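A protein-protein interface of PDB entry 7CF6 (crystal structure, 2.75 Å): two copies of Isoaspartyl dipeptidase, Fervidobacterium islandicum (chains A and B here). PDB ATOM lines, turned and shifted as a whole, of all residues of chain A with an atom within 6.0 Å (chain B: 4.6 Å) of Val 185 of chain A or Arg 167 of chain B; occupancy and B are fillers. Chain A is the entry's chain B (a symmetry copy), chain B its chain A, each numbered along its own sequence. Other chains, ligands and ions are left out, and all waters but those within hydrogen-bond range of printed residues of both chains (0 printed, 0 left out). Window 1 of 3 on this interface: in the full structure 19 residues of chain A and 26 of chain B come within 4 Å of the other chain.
The guanidinium group of Arg 184 of chain A is in hydrogen-bond range of a ring nitrogen (ND1) of His 166 of chain B, at 3.0 Å. The backbone carbonyl oxygen of Met 188 of chain A lies close to the backbone carbonyl oxygen of Glu 74 of chain B, at 3.5 Å.
OE1 of Glu 74 of chain B lies within salt-bridge range of NH1 of Arg 167 of chain B (3.4 Å). The side-chain carboxylate (OD1) of Asp 165 of chain B is in salt-bridge range of the guanidinium group (NE) of Arg 167 of chain B (2.9 Å). O of Asp 165 of chain B lies close to OG of Ser 168 of chain B (3.3 Å). The guanidinium group (NH2) of Arg 184 of chain A sits at hydrogen-bond distance from the side-chain sulfur (SD) of Met 188 of chain A.
Among the printed residues, pairs that only touch across the chains: Ala 181 of chain A with Ser 168 of chain B (3.5 Å), Ala 181 of chain A with Ser 169 of chain B (3.9 Å), Val 185 of chain A with Arg 167 of chain B (3.4 Å) and Met 188 of chain A with Phe 297 of chain B (3.5 Å).
Of the printed residues of chain A, Arg 167 of chain B touches Val 185. Printed residues of chain A within 4 Å of Ser 169 of chain B: Ala 181. Of the printed residues of chain B, Met 188 of chain A touches Glu 74 and Phe 297. Of the printed residues of chain A, Glu 74 of chain B touches Met 188 (3.5 Å). The nearest residue of chain A that does not touch Arg 167 of chain B is Met 188 of chain A (4.1 Å). The nearest printed residue of chain A that does not touch His 166 of chain B is Val 185 of chain A (4.7 Å).
Hydrophobic or aromatic side chains of chain B that line the printed part of chain A: His 166 and Phe 297.
No position is printed for both chains.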
ATOM      1  N   MET A 146     -30.576   0.960  13.295  1.00  0.00           N
ATOM      2  CA  MET A 146     -29.618   2.103  13.233  1.00  0.00           C
ATOM      3  C   MET A 146     -30.381   3.445  13.250  1.00  0.00           C
ATOM      4  O   MET A 146     -29.901   4.378  13.932  1.00  0.00           O
ATOM      5  CB  MET A 146     -28.688   2.050  12.007  1.00  0.00           C
ATOM      6  CG  MET A 146     -27.446   2.917  12.184  1.00  0.00           C
ATOM      7  SD  MET A 146     -26.608   3.402  10.666  1.00  0.00           S
ATOM      8  CE  MET A 146     -25.652   1.933  10.302  1.00  0.00           C
ATOM      9  N   ILE A 149     -31.816   4.140  17.003  1.00  0.00           N
ATOM     10  CA  ILE A 149     -30.827   4.550  18.048  1.00  0.00           C
ATOM     11  C   ILE A 149     -30.329   5.990  17.804  1.00  0.00           C
ATOM     12  O   ILE A 149     -29.844   6.659  18.782  1.00  0.00           O
ATOM     13  CB  ILE A 149     -29.655   3.546  18.106  1.00  0.00           C
ATOM     14  CG1 ILE A 149     -28.944   3.602  19.458  1.00  0.00           C
ATOM     15  CG2 ILE A 149     -28.685   3.783  16.958  1.00  0.00           C
ATOM     16  CD1 ILE A 149     -28.105   2.409  19.740  1.00  0.00           C
ATOM     17  N   VAL A 150     -30.387   6.451  16.557  1.00  0.00           N
ATOM     18  CA  VAL A 150     -29.960   7.825  16.154  1.00  0.00           C
ATOM     19  C   VAL A 150     -31.051   8.854  16.520  1.00  0.00           C
ATOM     20  O   VAL A 150     -30.670   9.999  16.874  1.00  0.00           O
ATOM     21  CB  VAL A 150     -29.574   7.855  14.657  1.00  0.00           C
ATOM     22  CG1 VAL A 150     -29.471   9.262  14.071  1.00  0.00           C
ATOM     23  CG2 VAL A 150     -28.272   7.094  14.430  1.00  0.00           C
ATOM     24  N   VAL A 180     -25.550  -6.495  14.713  1.00  0.00           N
ATOM     25  CA  VAL A 180     -24.514  -5.950  15.643  1.00  0.00           C
ATOM     26  C   VAL A 180     -23.717  -4.819  14.965  1.00  0.00           C
ATOM     27  O   VAL A 180     -23.317  -3.842  15.650  1.00  0.00           O
ATOM     28  CB  VAL A 180     -23.615  -7.092  16.148  1.00  0.00           C
ATOM     29  CG1 VAL A 180     -22.472  -6.554  16.991  1.00  0.00           C
ATOM     30  CG2 VAL A 180     -24.432  -8.133  16.922  1.00  0.00           C
ATOM     31  N   ALA A 181     -23.501  -4.888  13.653  1.00  0.00           N
ATOM     32  CA  ALA A 181     -22.719  -3.852  12.933  1.00  0.00           C
ATOM     33  C   ALA A 181     -23.505  -2.541  12.988  1.00  0.00           C
ATOM     34  O   ALA A 181     -22.920  -1.516  13.397  1.00  0.00           O
ATOM     35  CB  ALA A 181     -22.424  -4.285  11.518  1.00  0.00           C
ATOM     36  N   ASP A 182     -24.796  -2.629  12.634  1.00  0.00           N
ATOM     37  CA  ASP A 182     -25.793  -1.524  12.597  1.00  0.00           C
ATOM     38  C   ASP A 182     -25.888  -0.839  13.968  1.00  0.00           C
ATOM     39  O   ASP A 182     -25.844   0.391  14.012  1.00  0.00           O
ATOM     40  CB  ASP A 182     -27.173  -2.041  12.173  1.00  0.00           C
ATOM     41  CG  ASP A 182     -27.298  -2.331  10.684  1.00  0.00           C
ATOM     42  OD1 ASP A 182     -26.336  -2.009   9.941  1.00  0.00           O
ATOM     43  OD2 ASP A 182     -28.350  -2.880  10.284  1.00  0.00           O
ATOM     44  N   ILE A 183     -26.019  -1.581  15.061  1.00  0.00           N
ATOM     45  CA  ILE A 183     -26.250  -0.937  16.386  1.00  0.00           C
ATOM     46  C   ILE A 183     -24.932  -0.261  16.851  1.00  0.00           C
ATOM     47  O   ILE A 183     -24.985   0.824  17.489  1.00  0.00           O
ATOM     48  CB  ILE A 183     -26.868  -1.936  17.401  1.00  0.00           C
ATOM     49  CG1 ILE A 183     -27.840  -1.234  18.349  1.00  0.00           C
ATOM     50  CG2 ILE A 183     -25.803  -2.704  18.185  1.00  0.00           C
ATOM     51  CD1 ILE A 183     -29.061  -0.696  17.677  1.00  0.00           C
ATOM     52  N   ARG A 184     -23.773  -0.838  16.527  1.00  0.00           N
ATOM     53  CA  ARG A 184     -22.469  -0.186  16.809  1.00  0.00           C
ATOM     54  C   ARG A 184     -22.415   1.170  16.091  1.00  0.00           C
ATOM     55  O   ARG A 184     -22.292   2.186  16.793  1.00  0.00           O
ATOM     56  CB  ARG A 184     -21.279  -1.045  16.365  1.00  0.00           C
ATOM     57  CG  ARG A 184     -19.971  -0.270  16.394  1.00  0.00           C
ATOM     58  CD  ARG A 184     -18.781  -1.178  16.261  1.00  0.00           C
ATOM     59  NE  ARG A 184     -17.586  -0.388  16.023  1.00  0.00           N
ATOM     60  CZ  ARG A 184     -16.832   0.166  16.967  1.00  0.00           C
ATOM     61  NH1 ARG A 184     -17.141   0.006  18.241  1.00  0.00           N
ATOM     62  NH2 ARG A 184     -15.756   0.864  16.631  1.00  0.00           N
ATOM     63  N   VAL A 185     -22.470   1.179  14.751  1.00  0.00           N
ATOM     64  CA  VAL A 185     -22.283   2.421  13.952  1.00  0.00           C
ATOM     65  C   VAL A 185     -23.384   3.415  14.345  1.00  0.00           C
ATOM     66  O   VAL A 185     -23.052   4.609  14.570  1.00  0.00           O
ATOM     67  CB  VAL A 185     -22.254   2.115  12.451  1.00  0.00           C
ATOM     68  CG1 VAL A 185     -22.412   3.360  11.573  1.00  0.00           C
ATOM     69  CG2 VAL A 185     -20.990   1.353  12.101  1.00  0.00           C
ATOM     70  N   GLY A 186     -24.631   2.940  14.466  1.00  0.00           N
ATOM     71  CA  GLY A 186     -25.747   3.714  15.025  1.00  0.00           C
ATOM     72  C   GLY A 186     -25.391   4.304  16.376  1.00  0.00           C
ATOM     73  O   GLY A 186     -25.622   5.497  16.577  1.00  0.00           O
ATOM     74  N   GLY A 187     -24.832   3.515  17.285  1.00  0.00           N
ATOM     75  CA  GLY A 187     -24.318   4.028  18.569  1.00  0.00           C
ATOM     76  C   GLY A 187     -23.273   5.115  18.347  1.00  0.00           C
ATOM     77  O   GLY A 187     -23.448   6.228  18.881  1.00  0.00           O
ATOM     78  N   MET A 188     -22.242   4.830  17.550  1.00  0.00           N
ATOM     79  CA  MET A 188     -21.106   5.765  17.349  1.00  0.00           C
ATOM     80  C   MET A 188     -21.653   7.133  16.926  1.00  0.00           C
ATOM     81  O   MET A 188     -21.348   8.110  17.645  1.00  0.00           O
ATOM     82  CB  MET A 188     -20.118   5.251  16.302  1.00  0.00           C
ATOM     83  CG  MET A 188     -19.540   3.899  16.669  1.00  0.00           C
ATOM     84  SD  MET A 188     -18.394   3.284  15.428  1.00  0.00           S
ATOM     85  CE  MET A 188     -17.042   4.437  15.661  1.00  0.00           C
ATOM     86  N   ILE A 189     -22.464   7.182  15.856  1.00  0.00           N
ATOM     87  CA  ILE A 189     -23.119   8.414  15.307  1.00  0.00           C
ATOM     88  C   ILE A 189     -23.837   9.223  16.417  1.00  0.00           C
ATOM     89  O   ILE A 189     -23.680  10.491  16.442  1.00  0.00           O
ATOM     90  CB  ILE A 189     -24.079   8.060  14.153  1.00  0.00           C
ATOM     91  CG1 ILE A 189     -23.309   7.699  12.880  1.00  0.00           C
ATOM     92  CG2 ILE A 189     -25.069   9.187  13.900  1.00  0.00           C
ATOM     93  CD1 ILE A 189     -24.196   7.181  11.745  1.00  0.00           C
ATOM     94  N   SER A 190     -24.604   8.559  17.293  1.00  0.00           N
ATOM     95  CA  SER A 190     -25.496   9.234  18.269  1.00  0.00           C
ATOM     96  C   SER A 190     -24.813   9.463  19.631  1.00  0.00           C
ATOM     97  O   SER A 190     -25.447  10.085  20.508  1.00  0.00           O
ATOM     98  CB  SER A 190     -26.763   8.466  18.418  1.00  0.00           C
ATOM     99  OG  SER A 190     -26.592   7.439  19.365  1.00  0.00           O
ATOM    100  N   GLU B  74     -18.134  10.029  13.828  1.00  0.00           N
ATOM    101  CA  GLU B  74     -17.896   8.765  14.570  1.00  0.00           C
ATOM    102  C   GLU B  74     -17.814   9.039  16.081  1.00  0.00           C
ATOM    103  O   GLU B  74     -17.934   8.079  16.881  1.00  0.00           O
ATOM    104  CB  GLU B  74     -16.601   8.099  14.122  1.00  0.00           C
ATOM    105  CG  GLU B  74     -16.505   7.899  12.629  1.00  0.00           C
ATOM    106  CD  GLU B  74     -15.497   8.815  11.950  1.00  0.00           C
ATOM    107  OE1 GLU B  74     -15.318   8.679  10.685  1.00  0.00           O
ATOM    108  OE2 GLU B  74     -14.885   9.667  12.687  1.00  0.00           O
ATOM    109  N   THR B 103     -19.053   7.269   6.712  1.00  0.00           N
ATOM    110  CA  THR B 103     -19.588   6.507   7.867  1.00  0.00           C
ATOM    111  C   THR B 103     -21.068   6.862   8.074  1.00  0.00           C
ATOM    112  O   THR B 103     -21.887   5.896   8.116  1.00  0.00           O
ATOM    113  CB  THR B 103     -18.726   6.788   9.095  1.00  0.00           C
ATOM    114  OG1 THR B 103     -17.385   6.542   8.657  1.00  0.00           O
ATOM    115  CG2 THR B 103     -19.136   5.954  10.284  1.00  0.00           C
ATOM    116  N   TYR B 134     -20.527   3.948   2.923  1.00  0.00           N
ATOM    117  CA  TYR B 134     -19.995   2.839   3.761  1.00  0.00           C
ATOM    118  C   TYR B 134     -20.937   1.630   3.726  1.00  0.00           C
ATOM    119  O   TYR B 134     -20.502   0.546   3.316  1.00  0.00           O
ATOM    120  CB  TYR B 134     -19.840   3.285   5.221  1.00  0.00           C
ATOM    121  CG  TYR B 134     -18.481   3.775   5.652  1.00  0.00           C
ATOM    122  CD1 TYR B 134     -17.716   4.601   4.852  1.00  0.00           C
ATOM    123  CD2 TYR B 134     -17.952   3.411   6.882  1.00  0.00           C
ATOM    124  CE1 TYR B 134     -16.470   5.054   5.262  1.00  0.00           C
ATOM    125  CE2 TYR B 134     -16.703   3.851   7.308  1.00  0.00           C
ATOM    126  CZ  TYR B 134     -15.956   4.694   6.502  1.00  0.00           C
ATOM    127  OH  TYR B 134     -14.723   5.137   6.921  1.00  0.00           O
ATOM    128  N   ASP B 165     -13.378  -3.277   7.973  1.00  0.00           N
ATOM    129  CA  ASP B 165     -13.518  -2.085   8.867  1.00  0.00           C
ATOM    130  C   ASP B 165     -14.502  -2.434   9.990  1.00  0.00           C
ATOM    131  O   ASP B 165     -15.451  -3.247   9.732  1.00  0.00           O
ATOM    132  CB  ASP B 165     -13.959  -0.835   8.088  1.00  0.00           C
ATOM    133  CG  ASP B 165     -13.525   0.479   8.711  1.00  0.00           C
ATOM    134  OD1 ASP B 165     -14.278   1.006   9.554  1.00  0.00           O
ATOM    135  OD2 ASP B 165     -12.446   0.963   8.342  1.00  0.00           O
ATOM    136  N   HIS B 166     -14.283  -1.867  11.184  1.00  0.00           N
ATOM    137  CA  HIS B 166     -15.210  -2.023  12.340  1.00  0.00           C
ATOM    138  C   HIS B 166     -16.531  -1.290  12.062  1.00  0.00           C
ATOM    139  O   HIS B 166     -17.606  -1.834  12.452  1.00  0.00           O
ATOM    140  CB  HIS B 166     -14.533  -1.659  13.666  1.00  0.00           C
ATOM    141  CG  HIS B 166     -13.781  -0.369  13.724  1.00  0.00           C
ATOM    142  ND1 HIS B 166     -14.410   0.828  13.959  1.00  0.00           N
ATOM    143  CD2 HIS B 166     -12.458  -0.107  13.749  1.00  0.00           C
ATOM    144  CE1 HIS B 166     -13.515   1.783  14.061  1.00  0.00           C
ATOM    145  NE2 HIS B 166     -12.305   1.239  13.932  1.00  0.00           N
ATOM    146  N   ARG B 167     -16.464  -0.171  11.329  1.00  0.00           N
ATOM    147  CA  ARG B 167     -17.642   0.628  10.901  1.00  0.00           C
ATOM    148  C   ARG B 167     -18.324  -0.018   9.694  1.00  0.00           C
ATOM    149  O   ARG B 167     -19.319   0.519   9.245  1.00  0.00           O
ATOM    150  CB  ARG B 167     -17.246   2.071  10.561  1.00  0.00           C
ATOM    151  CG  ARG B 167     -16.736   2.893  11.739  1.00  0.00           C
ATOM    152  CD  ARG B 167     -15.883   4.070  11.310  1.00  0.00           C
ATOM    153  NE  ARG B 167     -14.688   3.653  10.570  1.00  0.00           N
ATOM    154  CZ  ARG B 167     -13.681   4.458  10.208  1.00  0.00           C
ATOM    155  NH1 ARG B 167     -13.703   5.746  10.515  1.00  0.00           N
ATOM    156  NH2 ARG B 167     -12.651   3.974   9.536  1.00  0.00           N
ATOM    157  N   SER B 168     -17.829  -1.125   9.162  1.00  0.00           N
ATOM    158  CA  SER B 168     -18.485  -1.793   8.003  1.00  0.00           C
ATOM    159  C   SER B 168     -19.789  -2.421   8.483  1.00  0.00           C
ATOM    160  O   SER B 168     -19.887  -2.711   9.694  1.00  0.00           O
ATOM    161  CB  SER B 168     -17.623  -2.841   7.341  1.00  0.00           C
ATOM    162  OG  SER B 168     -17.998  -4.143   7.784  1.00  0.00           O
ATOM    163  N   SER B 169     -20.704  -2.657   7.545  1.00  0.00           N
ATOM    164  CA  SER B 169     -21.972  -3.407   7.730  1.00  0.00           C
ATOM    165  C   SER B 169     -21.707  -4.918   7.703  1.00  0.00           C
ATOM    166  O   SER B 169     -22.693  -5.688   7.593  1.00  0.00           O
ATOM    167  CB  SER B 169     -22.951  -3.026   6.659  1.00  0.00           C
ATOM    168  OG  SER B 169     -24.187  -3.691   6.840  1.00  0.00           O
ATOM    169  N   HIS B 199     -13.628   1.639   0.419  1.00  0.00           N
ATOM    170  CA  HIS B 199     -12.989   2.067   1.690  1.00  0.00           C
ATOM    171  C   HIS B 199     -12.545   0.835   2.458  1.00  0.00           C
ATOM    172  O   HIS B 199     -13.417   0.098   2.920  1.00  0.00           O
ATOM    173  CB  HIS B 199     -13.939   2.832   2.595  1.00  0.00           C
ATOM    174  CG  HIS B 199     -13.375   3.011   3.961  1.00  0.00           C
ATOM    175  ND1 HIS B 199     -12.463   3.999   4.252  1.00  0.00           N
ATOM    176  CD2 HIS B 199     -13.580   2.327   5.106  1.00  0.00           C
ATOM    177  CE1 HIS B 199     -12.145   3.929   5.528  1.00  0.00           C
ATOM    178  NE2 HIS B 199     -12.816   2.914   6.076  1.00  0.00           N
ATOM    179  N   ARG B 231      -2.207   2.827   4.175  1.00  0.00           N
ATOM    180  CA  ARG B 231      -2.596   2.639   5.606  1.00  0.00           C
ATOM    181  C   ARG B 231      -1.468   1.980   6.406  1.00  0.00           C
ATOM    182  O   ARG B 231      -0.989   2.574   7.393  1.00  0.00           O
ATOM    183  CB  ARG B 231      -3.815   1.706   5.711  1.00  0.00           C
ATOM    184  CG  ARG B 231      -5.002   2.322   6.432  1.00  0.00           C
ATOM    185  CD  ARG B 231      -6.081   1.337   6.826  1.00  0.00           C
ATOM    186  NE  ARG B 231      -7.407   1.920   6.717  1.00  0.00           N
ATOM    187  CZ  ARG B 231      -7.780   3.066   7.282  1.00  0.00           C
ATOM    188  NH1 ARG B 231      -6.922   3.770   8.001  1.00  0.00           N
ATOM    189  NH2 ARG B 231      -9.009   3.534   7.118  1.00  0.00           N
ATOM    190  N   PRO B 295      -9.788   9.795  12.072  1.00  0.00           N
ATOM    191  CA  PRO B 295      -9.947   9.551  13.501  1.00  0.00           C
ATOM    192  C   PRO B 295      -8.841   8.659  14.085  1.00  0.00           C
ATOM    193  O   PRO B 295      -8.104   8.062  13.320  1.00  0.00           O
ATOM    194  CB  PRO B 295     -11.334   8.894  13.571  1.00  0.00           C
ATOM    195  CG  PRO B 295     -11.434   8.111  12.292  1.00  0.00           C
ATOM    196  CD  PRO B 295     -10.675   8.935  11.274  1.00  0.00           C
ATOM    197  N   PHE B 297      -8.946   5.581  17.075  1.00  0.00           N
ATOM    198  CA  PHE B 297      -9.683   4.656  17.978  1.00  0.00           C
ATOM    199  C   PHE B 297      -8.661   4.029  18.937  1.00  0.00           C
ATOM    200  O   PHE B 297      -7.546   3.712  18.463  1.00  0.00           O
ATOM    201  CB  PHE B 297     -10.455   3.602  17.171  1.00  0.00           C
ATOM    202  CG  PHE B 297     -11.451   4.184  16.205  1.00  0.00           C
ATOM    203  CD1 PHE B 297     -12.735   4.515  16.620  1.00  0.00           C
ATOM    204  CD2 PHE B 297     -11.093   4.445  14.889  1.00  0.00           C
ATOM    205  CE1 PHE B 297     -13.644   5.090  15.737  1.00  0.00           C
ATOM    206  CE2 PHE B 297     -12.004   5.017  14.007  1.00  0.00           C
ATOM    207  CZ  PHE B 297     -13.279   5.340  14.431  1.00  0.00           C
